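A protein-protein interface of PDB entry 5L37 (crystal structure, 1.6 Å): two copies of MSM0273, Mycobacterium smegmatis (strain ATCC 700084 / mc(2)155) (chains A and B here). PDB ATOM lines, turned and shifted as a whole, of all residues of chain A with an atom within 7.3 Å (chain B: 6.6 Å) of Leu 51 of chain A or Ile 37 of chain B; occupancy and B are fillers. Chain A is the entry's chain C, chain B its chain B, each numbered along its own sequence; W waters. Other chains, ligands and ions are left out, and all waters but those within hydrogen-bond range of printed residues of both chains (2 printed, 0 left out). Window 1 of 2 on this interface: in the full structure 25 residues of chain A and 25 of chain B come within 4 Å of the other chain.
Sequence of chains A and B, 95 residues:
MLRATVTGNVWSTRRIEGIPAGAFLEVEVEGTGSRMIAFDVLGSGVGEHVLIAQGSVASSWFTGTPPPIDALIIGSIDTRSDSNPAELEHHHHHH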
ATOM      1  N   MET A   1     -16.427  21.335   8.706  1.00  0.00           N
ATOM      2  CA  MET A   1     -17.056  22.666   8.462  1.00  0.00           C
ATOM      3  C   MET A   1     -17.922  22.560   7.224  1.00  0.00           C
ATOM      4  O   MET A   1     -17.782  21.646   6.414  1.00  0.00           O
ATOM      5  CB  MET A   1     -15.991  23.800   8.306  1.00  0.00           C
ATOM      6  CG  MET A   1     -15.215  24.129   9.616  1.00  0.00           C
ATOM      7  SD  MET A   1     -13.832  22.952   9.851  1.00  0.00           S
ATOM      8  CE  MET A   1     -12.667  23.543   8.591  1.00  0.00           C
ATOM      9  N   LEU A   2     -18.872  23.495   7.103  1.00  0.00           N
ATOM     10  CA  LEU A   2     -19.761  23.474   5.936  1.00  0.00           C
ATOM     11  C   LEU A   2     -19.793  24.831   5.245  1.00  0.00           C
ATOM     12  O   LEU A   2     -19.687  25.879   5.876  1.00  0.00           O
ATOM     13  CB  LEU A   2     -21.167  23.109   6.335  1.00  0.00           C
ATOM     14  CG  LEU A   2     -21.349  21.703   6.911  1.00  0.00           C
ATOM     15  CD1 LEU A   2     -22.747  21.584   7.501  1.00  0.00           C
ATOM     16  CD2 LEU A   2     -21.096  20.606   5.859  1.00  0.00           C
ATOM     17  N   ARG A   3     -19.926  24.803   3.932  1.00  0.00           N
ATOM     18  CA  ARG A   3     -20.246  26.003   3.155  1.00  0.00           C
ATOM     19  C   ARG A   3     -21.750  26.217   3.241  1.00  0.00           C
ATOM     20  O   ARG A   3     -22.524  25.268   3.053  1.00  0.00           O
ATOM     21  CB  ARG A   3     -19.802  25.835   1.685  1.00  0.00           C
ATOM     22  CG  ARG A   3     -18.327  25.662   1.505  1.00  0.00           C
ATOM     23  CD  ARG A   3     -17.939  25.596   0.027  1.00  0.00           C
ATOM     24  NE  ARG A   3     -18.660  24.594  -0.721  1.00  0.00           N
ATOM     25  CZ  ARG A   3     -19.611  24.870  -1.617  1.00  0.00           C
ATOM     26  NH1 ARG A   3     -19.965  26.125  -1.885  1.00  0.00           N
ATOM     27  NH2 ARG A   3     -20.206  23.876  -2.256  1.00  0.00           N
ATOM     28  N   ALA A   4     -22.150  27.461   3.469  1.00  0.00           N
ATOM     29  CA  ALA A   4     -23.564  27.802   3.534  1.00  0.00           C
ATOM     30  C   ALA A   4     -23.779  29.180   2.981  1.00  0.00           C
ATOM     31  O   ALA A   4     -22.806  29.930   2.764  1.00  0.00           O
ATOM     32  CB  ALA A   4     -24.039  27.741   4.968  1.00  0.00           C
ATOM     33  N   THR A   5     -25.043  29.505   2.739  1.00  0.00           N
ATOM     34  CA  THR A   5     -25.430  30.823   2.266  1.00  0.00           C
ATOM     35  C   THR A   5     -26.337  31.435   3.304  1.00  0.00           C
ATOM     36  O   THR A   5     -27.291  30.781   3.741  1.00  0.00           O
ATOM     37  CB  THR A   5     -26.160  30.746   0.894  1.00  0.00           C
ATOM     38  OG1 THR A   5     -25.283  30.109  -0.049  1.00  0.00           O
ATOM     39  CG2 THR A   5     -26.528  32.134   0.389  1.00  0.00           C
ATOM     40  N   ALA A  38     -27.015  29.947  12.562  1.00  0.00           N
ATOM     41  CA  ALA A  38     -25.630  30.067  12.966  1.00  0.00           C
ATOM     42  C   ALA A  38     -25.379  31.402  13.596  1.00  0.00           C
ATOM     43  O   ALA A  38     -25.981  32.409  13.183  1.00  0.00           O
ATOM     44  CB  ALA A  38     -24.674  29.878  11.743  1.00  0.00           C
ATOM     45  N   LEU A  42     -19.029  38.416  12.474  1.00  0.00           N
ATOM     46  CA  LEU A  42     -18.352  39.108  11.359  1.00  0.00           C
ATOM     47  C   LEU A  42     -19.166  40.148  10.589  1.00  0.00           C
ATOM     48  O   LEU A  42     -18.662  40.727   9.617  1.00  0.00           O
ATOM     49  CB  LEU A  42     -17.818  38.071  10.373  1.00  0.00           C
ATOM     50  CG  LEU A  42     -16.662  37.230  10.933  1.00  0.00           C
ATOM     51  CD1 LEU A  42     -16.320  36.060   9.948  1.00  0.00           C
ATOM     52  CD2 LEU A  42     -15.421  38.098  11.225  1.00  0.00           C
ATOM     53  N   GLU A  48     -24.635  36.105   1.319  1.00  0.00           N
ATOM     54  CA  GLU A  48     -23.208  35.841   1.416  1.00  0.00           C
ATOM     55  C   GLU A  48     -22.895  34.360   1.619  1.00  0.00           C
ATOM     56  O   GLU A  48     -23.595  33.638   2.323  1.00  0.00           O
ATOM     57  CB  GLU A  48     -22.621  36.621   2.581  1.00  0.00           C
ATOM     58  CG  GLU A  48     -21.137  36.519   2.726  1.00  0.00           C
ATOM     59  CD  GLU A  48     -20.630  37.462   3.807  1.00  0.00           C
ATOM     60  OE1 GLU A  48     -21.389  38.375   4.220  1.00  0.00           O
ATOM     61  OE2 GLU A  48     -19.482  37.273   4.265  1.00  0.00           O
ATOM     62  N   HIS A  49     -21.843  33.901   0.971  1.00  0.00           N
ATOM     63  CA  HIS A  49     -21.401  32.538   1.147  1.00  0.00           C
ATOM     64  C   HIS A  49     -20.387  32.453   2.264  1.00  0.00           C
ATOM     65  O   HIS A  49     -19.359  33.131   2.215  1.00  0.00           O
ATOM     66  CB  HIS A  49     -20.807  32.008  -0.157  1.00  0.00           C
ATOM     67  CG  HIS A  49     -21.752  32.127  -1.301  1.00  0.00           C
ATOM     68  ND1 HIS A  49     -22.899  31.382  -1.391  1.00  0.00           N
ATOM     69  CD2 HIS A  49     -21.725  32.923  -2.400  1.00  0.00           C
ATOM     70  CE1 HIS A  49     -23.565  31.733  -2.482  1.00  0.00           C
ATOM     71  NE2 HIS A  49     -22.864  32.653  -3.118  1.00  0.00           N
ATOM     72  N   VAL A  50     -20.663  31.594   3.242  1.00  0.00           N
ATOM     73  CA  VAL A  50     -19.872  31.572   4.471  1.00  0.00           C
ATOM     74  C   VAL A  50     -19.463  30.146   4.826  1.00  0.00           C
ATOM     75  O   VAL A  50     -20.012  29.181   4.305  1.00  0.00           O
ATOM     76  CB  VAL A  50     -20.642  32.173   5.664  1.00  0.00           C
ATOM     77  CG1 VAL A  50     -20.943  33.670   5.417  1.00  0.00           C
ATOM     78  CG2 VAL A  50     -21.943  31.441   5.875  1.00  0.00           C
ATOM     79  N   LEU A  51     -18.501  30.053   5.733  1.00  0.00           N
ATOM     80  CA  LEU A  51     -17.970  28.803   6.256  1.00  0.00           C
ATOM     81  C   LEU A  51     -18.408  28.688   7.718  1.00  0.00           C
ATOM     82  O   LEU A  51     -18.220  29.635   8.473  1.00  0.00           O
ATOM     83  CB  LEU A  51     -16.446  28.837   6.155  1.00  0.00           C
ATOM     84  CG  LEU A  51     -15.677  27.571   6.458  1.00  0.00           C
ATOM     85  CD1 LEU A  51     -16.161  26.474   5.431  1.00  0.00           C
ATOM     86  CD2 LEU A  51     -14.185  27.897   6.355  1.00  0.00           C
ATOM     87  N   ILE A  52     -19.010  27.565   8.096  1.00  0.00           N
ATOM     88  CA  ILE A  52     -19.558  27.364   9.440  1.00  0.00           C
ATOM     89  C   ILE A  52     -18.863  26.236  10.156  1.00  0.00           C
ATOM     90  O   ILE A  52     -18.637  25.164   9.549  1.00  0.00           O
ATOM     91  CB  ILE A  52     -21.058  27.053   9.367  1.00  0.00           C
ATOM     92  CG1 ILE A  52     -21.718  28.360   8.864  1.00  0.00           C
ATOM     93  CG2 ILE A  52     -21.600  26.646  10.745  1.00  0.00           C
ATOM     94  CD1 ILE A  52     -23.115  28.168   8.520  1.00  0.00           C
ATOM     95  N   ALA A  53     -18.560  26.446  11.434  1.00  0.00           N
ATOM     96  CA  ALA A  53     -18.122  25.334  12.317  1.00  0.00           C
ATOM     97  C   ALA A  53     -19.215  25.016  13.316  1.00  0.00           C
ATOM     98  O   ALA A  53     -19.951  25.919  13.745  1.00  0.00           O
ATOM     99  CB  ALA A  53     -16.843  25.700  13.054  1.00  0.00           C
ATOM    100  N   LEU A  72     -21.180  28.475  14.324  1.00  0.00           N
ATOM    101  CA  LEU A  72     -20.501  29.780  14.244  1.00  0.00           C
ATOM    102  C   LEU A  72     -19.995  29.964  12.842  1.00  0.00           C
ATOM    103  O   LEU A  72     -19.331  29.099  12.300  1.00  0.00           O
ATOM    104  CB  LEU A  72     -19.321  29.849  15.232  1.00  0.00           C
ATOM    105  CG  LEU A  72     -18.477  31.128  15.218  1.00  0.00           C
ATOM    106  CD1 LEU A  72     -19.314  32.366  15.688  1.00  0.00           C
ATOM    107  CD2 LEU A  72     -17.292  30.900  16.143  1.00  0.00           C
ATOM    108  N   ILE A  73     -20.292  31.130  12.265  1.00  0.00           N
ATOM    109  CA  ILE A  73     -19.667  31.490  10.996  1.00  0.00           C
ATOM    110  C   ILE A  73     -18.219  31.890  11.227  1.00  0.00           C
ATOM    111  O   ILE A  73     -17.930  32.792  12.026  1.00  0.00           O
ATOM    112  CB  ILE A  73     -20.485  32.618  10.338  1.00  0.00           C
ATOM    113  CG1 ILE A  73     -21.783  32.020   9.764  1.00  0.00           C
ATOM    114  CG2 ILE A  73     -19.635  33.328   9.244  1.00  0.00           C
ATOM    115  CD1 ILE A  73     -22.902  33.129   9.465  1.00  0.00           C
ATOM    116  N   ILE A  74     -17.288  31.203  10.564  1.00  0.00           N
ATOM    117  CA  ILE A  74     -15.883  31.497  10.836  1.00  0.00           C
ATOM    118  C   ILE A  74     -15.229  32.295   9.712  1.00  0.00           C
ATOM    119  O   ILE A  74     -14.081  32.706   9.861  1.00  0.00           O
ATOM    120  CB  ILE A  74     -15.031  30.196  11.157  1.00  0.00           C
ATOM    121  CG1 ILE A  74     -14.990  29.275   9.972  1.00  0.00           C
ATOM    122  CG2 ILE A  74     -15.591  29.473  12.385  1.00  0.00           C
ATOM    123  CD1 ILE A  74     -13.993  28.099  10.206  1.00  0.00           C
ATOM    124  N   GLY A  75     -15.923  32.497   8.588  1.00  0.00           N
ATOM    125  CA  GLY A  75     -15.332  33.331   7.529  1.00  0.00           C
ATOM    126  C   GLY A  75     -16.222  33.347   6.294  1.00  0.00           C
ATOM    127  O   GLY A  75     -17.201  32.580   6.205  1.00  0.00           O
ATOM    128  N   SER A  76     -15.917  34.232   5.357  1.00  0.00           N
ATOM    129  CA  SER A  76     -16.634  34.197   4.079  1.00  0.00           C
ATOM    130  C   SER A  76     -15.785  33.476   3.065  1.00  0.00           C
ATOM    131  O   SER A  76     -14.571  33.337   3.245  1.00  0.00           O
ATOM    132  CB  SER A  76     -17.046  35.597   3.589  1.00  0.00           C
ATOM    133  OG  SER A  76     -15.914  36.357   3.359  1.00  0.00           O
ATOM    134  N   ILE A  77     -16.426  32.947   2.026  1.00  0.00           N
ATOM    135  CA  ILE A  77     -15.724  32.131   1.031  1.00  0.00           C
ATOM    136  C   ILE A  77     -15.292  33.010  -0.142  1.00  0.00           C
ATOM    137  O   ILE A  77     -16.122  33.676  -0.797  1.00  0.00           O
ATOM    138  CB  ILE A  77     -16.628  31.009   0.544  1.00  0.00           C
ATOM    139  CG1 ILE A  77     -17.031  30.149   1.760  1.00  0.00           C
ATOM    140  CG2 ILE A  77     -15.972  30.172  -0.534  1.00  0.00           C
ATOM    141  CD1 ILE A  77     -18.074  29.178   1.464  1.00  0.00           C
ATOM    142  N   ASP A  82     -12.568  26.579  -5.085  1.00  0.00           N
ATOM    143  CA  ASP A  82     -13.023  25.695  -6.150  1.00  0.00           C
ATOM    144  C   ASP A  82     -13.530  24.357  -5.583  1.00  0.00           C
ATOM    145  O   ASP A  82     -13.344  24.019  -4.391  1.00  0.00           O
ATOM    146  CB  ASP A  82     -11.925  25.461  -7.195  1.00  0.00           C
ATOM    147  CG  ASP A  82     -10.598  24.938  -6.600  1.00  0.00           C
ATOM    148  OD1 ASP A  82     -10.634  24.054  -5.745  1.00  0.00           O
ATOM    149  OD2 ASP A  82      -9.520  25.398  -7.042  1.00  0.00           O
ATOM    150  N   GLY B   8     -11.260  19.959  -3.569  1.00  0.00           N
ATOM    151  CA  GLY B   8     -11.017  21.354  -3.917  1.00  0.00           C
ATOM    152  C   GLY B   8     -10.381  22.150  -2.782  1.00  0.00           C
ATOM    153  O   GLY B   8     -10.193  21.655  -1.677  1.00  0.00           O
ATOM    154  N   VAL B  10     -10.515  25.758  -0.553  1.00  0.00           N
ATOM    155  CA  VAL B  10     -11.352  26.867  -0.114  1.00  0.00           C
ATOM    156  C   VAL B  10     -10.468  27.938   0.506  1.00  0.00           C
ATOM    157  O   VAL B  10      -9.672  27.643   1.400  1.00  0.00           O
ATOM    158  CB  VAL B  10     -12.380  26.398   0.910  1.00  0.00           C
ATOM    159  CG1 VAL B  10     -13.104  27.593   1.585  1.00  0.00           C
ATOM    160  CG2 VAL B  10     -13.360  25.444   0.222  1.00  0.00           C
ATOM    161  N   SER B  12     -10.551  31.570   2.569  1.00  0.00           N
ATOM    162  CA  SER B  12     -11.392  32.478   3.327  1.00  0.00           C
ATOM    163  C   SER B  12     -10.488  33.572   3.804  1.00  0.00           C
ATOM    164  O   SER B  12      -9.827  33.371   4.855  1.00  0.00           O
ATOM    165  CB  SER B  12     -12.068  31.745   4.500  1.00  0.00           C
ATOM    166  OG  SER B  12     -12.933  32.613   5.222  1.00  0.00           O
ATOM    167  N   ILE B  19      -7.555  31.075  13.745  1.00  0.00           N
ATOM    168  CA  ILE B  19      -7.324  29.908  12.909  1.00  0.00           C
ATOM    169  C   ILE B  19      -5.804  29.695  12.695  1.00  0.00           C
ATOM    170  O   ILE B  19      -5.114  30.622  12.304  1.00  0.00           O
ATOM    171  CB  ILE B  19      -8.051  30.063  11.571  1.00  0.00           C
ATOM    172  CG1 ILE B  19      -9.564  30.137  11.859  1.00  0.00           C
ATOM    173  CG2 ILE B  19      -7.709  28.905  10.636  1.00  0.00           C
ATOM    174  CD1 ILE B  19     -10.343  30.620  10.719  1.00  0.00           C
ATOM    175  N   ALA B  23      -4.641  24.662   5.691  1.00  0.00           N
ATOM    176  CA  ALA B  23      -5.509  24.911   4.541  1.00  0.00           C
ATOM    177  C   ALA B  23      -6.916  24.420   4.775  1.00  0.00           C
ATOM    178  O   ALA B  23      -7.144  23.500   5.526  1.00  0.00           O
ATOM    179  CB  ALA B  23      -4.921  24.239   3.283  1.00  0.00           C
ATOM    180  N   PHE B  24      -7.893  25.061   4.145  1.00  0.00           N
ATOM    181  CA  PHE B  24      -9.262  24.552   4.113  1.00  0.00           C
ATOM    182  C   PHE B  24      -9.414  23.780   2.814  1.00  0.00           C
ATOM    183  O   PHE B  24      -9.136  24.332   1.719  1.00  0.00           O
ATOM    184  CB  PHE B  24     -10.299  25.698   4.137  1.00  0.00           C
ATOM    185  CG  PHE B  24     -10.309  26.510   5.411  1.00  0.00           C
ATOM    186  CD1 PHE B  24     -10.689  25.965   6.614  1.00  0.00           C
ATOM    187  CD2 PHE B  24      -9.999  27.839   5.369  1.00  0.00           C
ATOM    188  CE1 PHE B  24     -10.727  26.744   7.772  1.00  0.00           C
ATOM    189  CE2 PHE B  24     -10.044  28.642   6.521  1.00  0.00           C
ATOM    190  CZ  PHE B  24     -10.390  28.083   7.712  1.00  0.00           C
ATOM    191  N   LEU B  25      -9.764  22.516   2.923  1.00  0.00           N
ATOM    192  CA  LEU B  25      -9.965  21.677   1.767  1.00  0.00           C
ATOM    193  C   LEU B  25     -11.385  21.166   1.708  1.00  0.00           C
ATOM    194  O   LEU B  25     -11.924  20.669   2.721  1.00  0.00           O
ATOM    195  CB  LEU B  25      -8.979  20.484   1.845  1.00  0.00           C
ATOM    196  CG  LEU B  25      -7.472  20.815   1.852  1.00  0.00           C
ATOM    197  CD1 LEU B  25      -6.672  19.491   1.880  1.00  0.00           C
ATOM    198  CD2 LEU B  25      -7.036  21.647   0.619  1.00  0.00           C
ATOM    199  N   GLU B  26     -11.955  21.173   0.504  1.00  0.00           N
ATOM    200  CA  GLU B  26     -13.235  20.488   0.288  1.00  0.00           C
ATOM    201  C   GLU B  26     -12.941  19.017   0.143  1.00  0.00           C
ATOM    202  O   GLU B  26     -11.970  18.665  -0.512  1.00  0.00           O
ATOM    203  CB  GLU B  26     -13.929  20.976  -0.967  1.00  0.00           C
ATOM    204  CG  GLU B  26     -15.337  20.372  -1.100  1.00  0.00           C
ATOM    205  CD  GLU B  26     -15.962  20.750  -2.426  1.00  0.00           C
ATOM    206  OE1 GLU B  26     -15.594  20.120  -3.425  1.00  0.00           O
ATOM    207  OE2 GLU B  26     -16.720  21.756  -2.475  1.00  0.00           O
ATOM    208  N   VAL B  27     -13.743  18.179   0.788  1.00  0.00           N
ATOM    209  CA  VAL B  27     -13.590  16.726   0.656  1.00  0.00           C
ATOM    210  C   VAL B  27     -14.940  16.128   0.360  1.00  0.00           C
ATOM    211  O   VAL B  27     -15.970  16.689   0.744  1.00  0.00           O
ATOM    212  CB  VAL B  27     -12.996  16.070   1.926  1.00  0.00           C
ATOM    213  CG1 VAL B  27     -11.635  16.712   2.280  1.00  0.00           C
ATOM    214  CG2 VAL B  27     -13.987  16.158   3.124  1.00  0.00           C
ATOM    215  N   ARG B  35     -20.419  16.234   1.088  1.00  0.00           N
ATOM    216  CA  ARG B  35     -19.268  17.107   1.095  1.00  0.00           C
ATOM    217  C   ARG B  35     -19.151  17.855   2.395  1.00  0.00           C
ATOM    218  O   ARG B  35     -20.165  18.093   3.096  1.00  0.00           O
ATOM    219  CB  ARG B  35     -19.364  18.078  -0.057  1.00  0.00           C
ATOM    220  CG  ARG B  35     -19.242  17.327  -1.353  1.00  0.00           C
ATOM    221  CD  ARG B  35     -19.337  18.224  -2.516  1.00  0.00           C
ATOM    222  NE  ARG B  35     -19.174  17.473  -3.746  1.00  0.00           N
ATOM    223  CZ  ARG B  35     -18.142  17.599  -4.560  1.00  0.00           C
ATOM    224  NH1 ARG B  35     -17.176  18.461  -4.289  1.00  0.00           N
ATOM    225  NH2 ARG B  35     -18.104  16.882  -5.661  1.00  0.00           N
ATOM    226  N   MET B  36     -17.905  18.178   2.734  1.00  0.00           N
ATOM    227  CA  MET B  36     -17.654  19.062   3.857  1.00  0.00           C
ATOM    228  C   MET B  36     -16.328  19.754   3.609  1.00  0.00           C
ATOM    229  O   MET B  36     -15.579  19.416   2.674  1.00  0.00           O
ATOM    230  CB  MET B  36     -17.663  18.312   5.187  1.00  0.00           C
ATOM    231  CG  MET B  36     -16.385  17.539   5.437  1.00  0.00           C
ATOM    232  SD  MET B  36     -16.442  16.608   7.018  1.00  0.00           S
ATOM    233  CE  MET B  36     -17.648  15.425   6.521  1.00  0.00           C
ATOM    234  N   ILE B  37     -16.037  20.740   4.440  1.00  0.00           N
ATOM    235  CA  ILE B  37     -14.771  21.400   4.373  1.00  0.00           C
ATOM    236  C   ILE B  37     -13.931  20.949   5.589  1.00  0.00           C
ATOM    237  O   ILE B  37     -14.389  21.084   6.745  1.00  0.00           O
ATOM    238  CB  ILE B  37     -14.939  22.940   4.369  1.00  0.00           C
ATOM    239  CG1 ILE B  37     -15.824  23.402   3.201  1.00  0.00           C
ATOM    240  CG2 ILE B  37     -13.552  23.626   4.289  1.00  0.00           C
ATOM    241  CD1 ILE B  37     -15.344  22.964   1.829  1.00  0.00           C
ATOM    242  N   ALA B  38     -12.734  20.421   5.355  1.00  0.00           N
ATOM    243  CA  ALA B  38     -11.896  19.948   6.457  1.00  0.00           C
ATOM    244  C   ALA B  38     -10.630  20.750   6.518  1.00  0.00           C
ATOM    245  O   ALA B  38     -10.159  21.268   5.479  1.00  0.00           O
ATOM    246  CB  ALA B  38     -11.560  18.452   6.285  1.00  0.00           C
ATOM    247  N   PHE B  39     -10.096  20.921   7.714  1.00  0.00           N
ATOM    248  CA  PHE B  39      -8.819  21.607   7.864  1.00  0.00           C
ATOM    249  C   PHE B  39      -7.668  20.636   7.612  1.00  0.00           C
ATOM    250  O   PHE B  39      -7.776  19.438   7.932  1.00  0.00           O
ATOM    251  CB  PHE B  39      -8.711  22.220   9.261  1.00  0.00           C
ATOM    252  CG  PHE B  39      -7.679  23.295   9.363  1.00  0.00           C
ATOM    253  CD1 PHE B  39      -7.924  24.558   8.820  1.00  0.00           C
ATOM    254  CD2 PHE B  39      -6.469  23.050  10.001  1.00  0.00           C
ATOM    255  CE1 PHE B  39      -6.973  25.589   8.906  1.00  0.00           C
ATOM    256  CE2 PHE B  39      -5.492  24.081  10.066  1.00  0.00           C
ATOM    257  CZ  PHE B  39      -5.766  25.358   9.535  1.00  0.00           C
ATOM    258  N   ASP B  70     -13.906  22.019  13.233  1.00  0.00           N
ATOM    259  CA  ASP B  70     -14.637  20.780  13.626  1.00  0.00           C
ATOM    260  C   ASP B  70     -14.425  19.605  12.667  1.00  0.00           C
ATOM    261  O   ASP B  70     -15.173  18.655  12.711  1.00  0.00           O
ATOM    262  CB  ASP B  70     -16.139  21.072  13.745  1.00  0.00           C
ATOM    263  CG  ASP B  70     -16.753  21.480  12.417  1.00  0.00           C
ATOM    264  OD1 ASP B  70     -16.024  21.501  11.415  1.00  0.00           O
ATOM    265  OD2 ASP B  70     -17.976  21.720  12.348  1.00  0.00           O
ATOM    266  N   ALA B  71     -13.402  19.708  11.812  1.00  0.00           N
ATOM    267  CA  ALA B  71     -13.069  18.638  10.852  1.00  0.00           C
ATOM    268  C   ALA B  71     -11.605  18.797  10.497  1.00  0.00           C
ATOM    269  O   ALA B  71     -11.164  19.896  10.137  1.00  0.00           O
ATOM    270  CB  ALA B  71     -13.943  18.724   9.588  1.00  0.00           C
ATOM    271  N   LEU B  72     -10.864  17.688  10.660  1.00  0.00           N
ATOM    272  CA  LEU B  72      -9.408  17.698  10.501  1.00  0.00           C
ATOM    273  C   LEU B  72      -8.995  16.466   9.734  1.00  0.00           C
ATOM    274  O   LEU B  72      -9.404  15.353  10.076  1.00  0.00           O
ATOM    275  CB  LEU B  72      -8.731  17.725  11.880  1.00  0.00           C
ATOM    276  CG  LEU B  72      -7.196  17.673  11.911  1.00  0.00           C
ATOM    277  CD1 LEU B  72      -6.563  18.929  11.244  1.00  0.00           C
ATOM    278  CD2 LEU B  72      -6.705  17.577  13.374  1.00  0.00           C
HETATM  279  O   HOH W   1     -18.833  22.158  -0.498  1.00  0.00           O
HETATM  280  O   HOH W   2     -19.828  21.186  -3.925  1.00  0.00           O
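O of Phe 24 of chain B sits at hydrogen-bond distance from N of Val 10 of chain B, at 3.0 Å.
The side-chain carboxylate (OE1) of Glu 26 of chain B is in salt-bridge range of the guanidinium group (NH1) of Arg 35 of chain B, at 2.4 Å.
O of Met 36 of chain B lies within hydrogen-bond range of N of Val 27 of chain B.
The backbone NH of Ile 52 of chain A sits at hydrogen-bond distance from the backbone carbonyl oxygen of Leu 2 of chain A.
The backbone carbonyl oxygen (O) of Leu 51 of chain A lies within hydrogen-bond range of the backbone NH (N) of Ile 74 of chain A (2.8 Å).
The backbone NH of Ala 53 of chain A lies within hydrogen-bond range of the backbone carbonyl oxygen of Leu 72 of chain A, at 2.9 Å.
2 positions are printed for both chains.
Of the 15 pairs that touch across the chains among the printed residues, none has its exchanged pair printed and touching as well.
Of the 17 printed residues of chain B, 10 touch a printed residue of chain A.
Hydrophobic or aromatic side chains of chain B within 4 Å of the printed part of chain A: Phe 24, Met 36, Ile 37 and Ala 71.
Of the 20 printed residues of chain A, 8 touch a printed residue of chain B.
Hydrophobic or aromatic side chains of chain A that line the printed part of chain B: Met 1, Leu 2 and Leu 51.
Along chain A the printed residues that touch a printed residue of chain B span positions 1 to 82.
Among the printed residues, Asp or Glu carboxylates within 4 Å of a Lys or Arg side-chain nitrogen of the other chain: Arg 3 of chain A with Glu 26 of chain B (3.9 Å).
The side-chain hydroxyl of Ser 12 of chain B is in hydrogen-bond range of the backbone carbonyl oxygen of Ser 76 of chain A (2.7 Å).
NE of Arg 3 of chain A is in salt-bridge range of OE2 of Glu 26 of chain B.
N of Ile 37 of chain B is in hydrogen-bond range of O of Met 1 of chain A, 2.8 Å away.
N of Met 1 of chain A is in hydrogen-bond range of OD1 of Asp 70 of chain B, 2.7 Å away.
Among the printed residues, pairs that only touch across the chains: Met 1 of chain A with Phe 24 of chain B, Met 1 of chain A with Met 36 of chain B, Met 1 of chain A with Phe 39 of chain B, Met 1 of chain A with Ala 71 of chain B, Leu 2 of chain A with Arg 35 of chain B, Arg 3 of chain A with Ile 37 of chain B, Leu 51 of chain A with Phe 24 of chain B, Leu 51 of chain A with Ile 37 of chain B, Ala 53 of chain A with Asp 70 of chain B, Gly 75 of chain A with Ser 12 of chain B and Asp 82 of chain A with Gly 8 of chain B.
Water W1 bridges the guanidinium group (NE) of Arg 3 of chain A (2.5 Å) and the side-chain carboxylate (OE2) of Glu 26 of chain B (2.9 Å).
Water W2 lies within hydrogen-bond range of the guanidinium group (NH2) of Arg 3 of chain A (3.2 Å) and the side-chain carboxylate (OE2) of Glu 26 of chain B (3.5 Å).
Val 50 of chain A touches none of the printed residues of chain B.
Of chain B, only Phe 24 (3.9 Å) and Ile 37 (3.8 Å) come within 4 Å of Leu 51 of chain A.
Of the printed residues of chain B, Ala 53 of chain A touches Asp 70 (3.6 Å).
Of the printed residues of chain A, Gly 8 of chain B touches Asp 82.
Leu 25 of chain B touches none of the printed residues of chain A.
Of chain A, only Met 1, Arg 3 and Leu 51 come within 4 Å of Ile 37 of chain B.
Of the printed residues of chain A, Phe 39 of chain B touches Met 1 (3.8 Å).
Printed residues of chain A within 4 Å of Asp 70 of chain B: Met 1 (2.7 Å) and Ala 53 (3.6 Å).
Printed residues of chain A within 4 Å of Ala 71 of chain B: Met 1 (3.7 Å).
The nearest residue of chain B that does not touch Leu 51 of chain A is Ser 12 of chain B (4.8 Å).
The nearest residue of chain A that does not touch Ile 37 of chain B is Leu 2 of chain A (4.7 Å).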
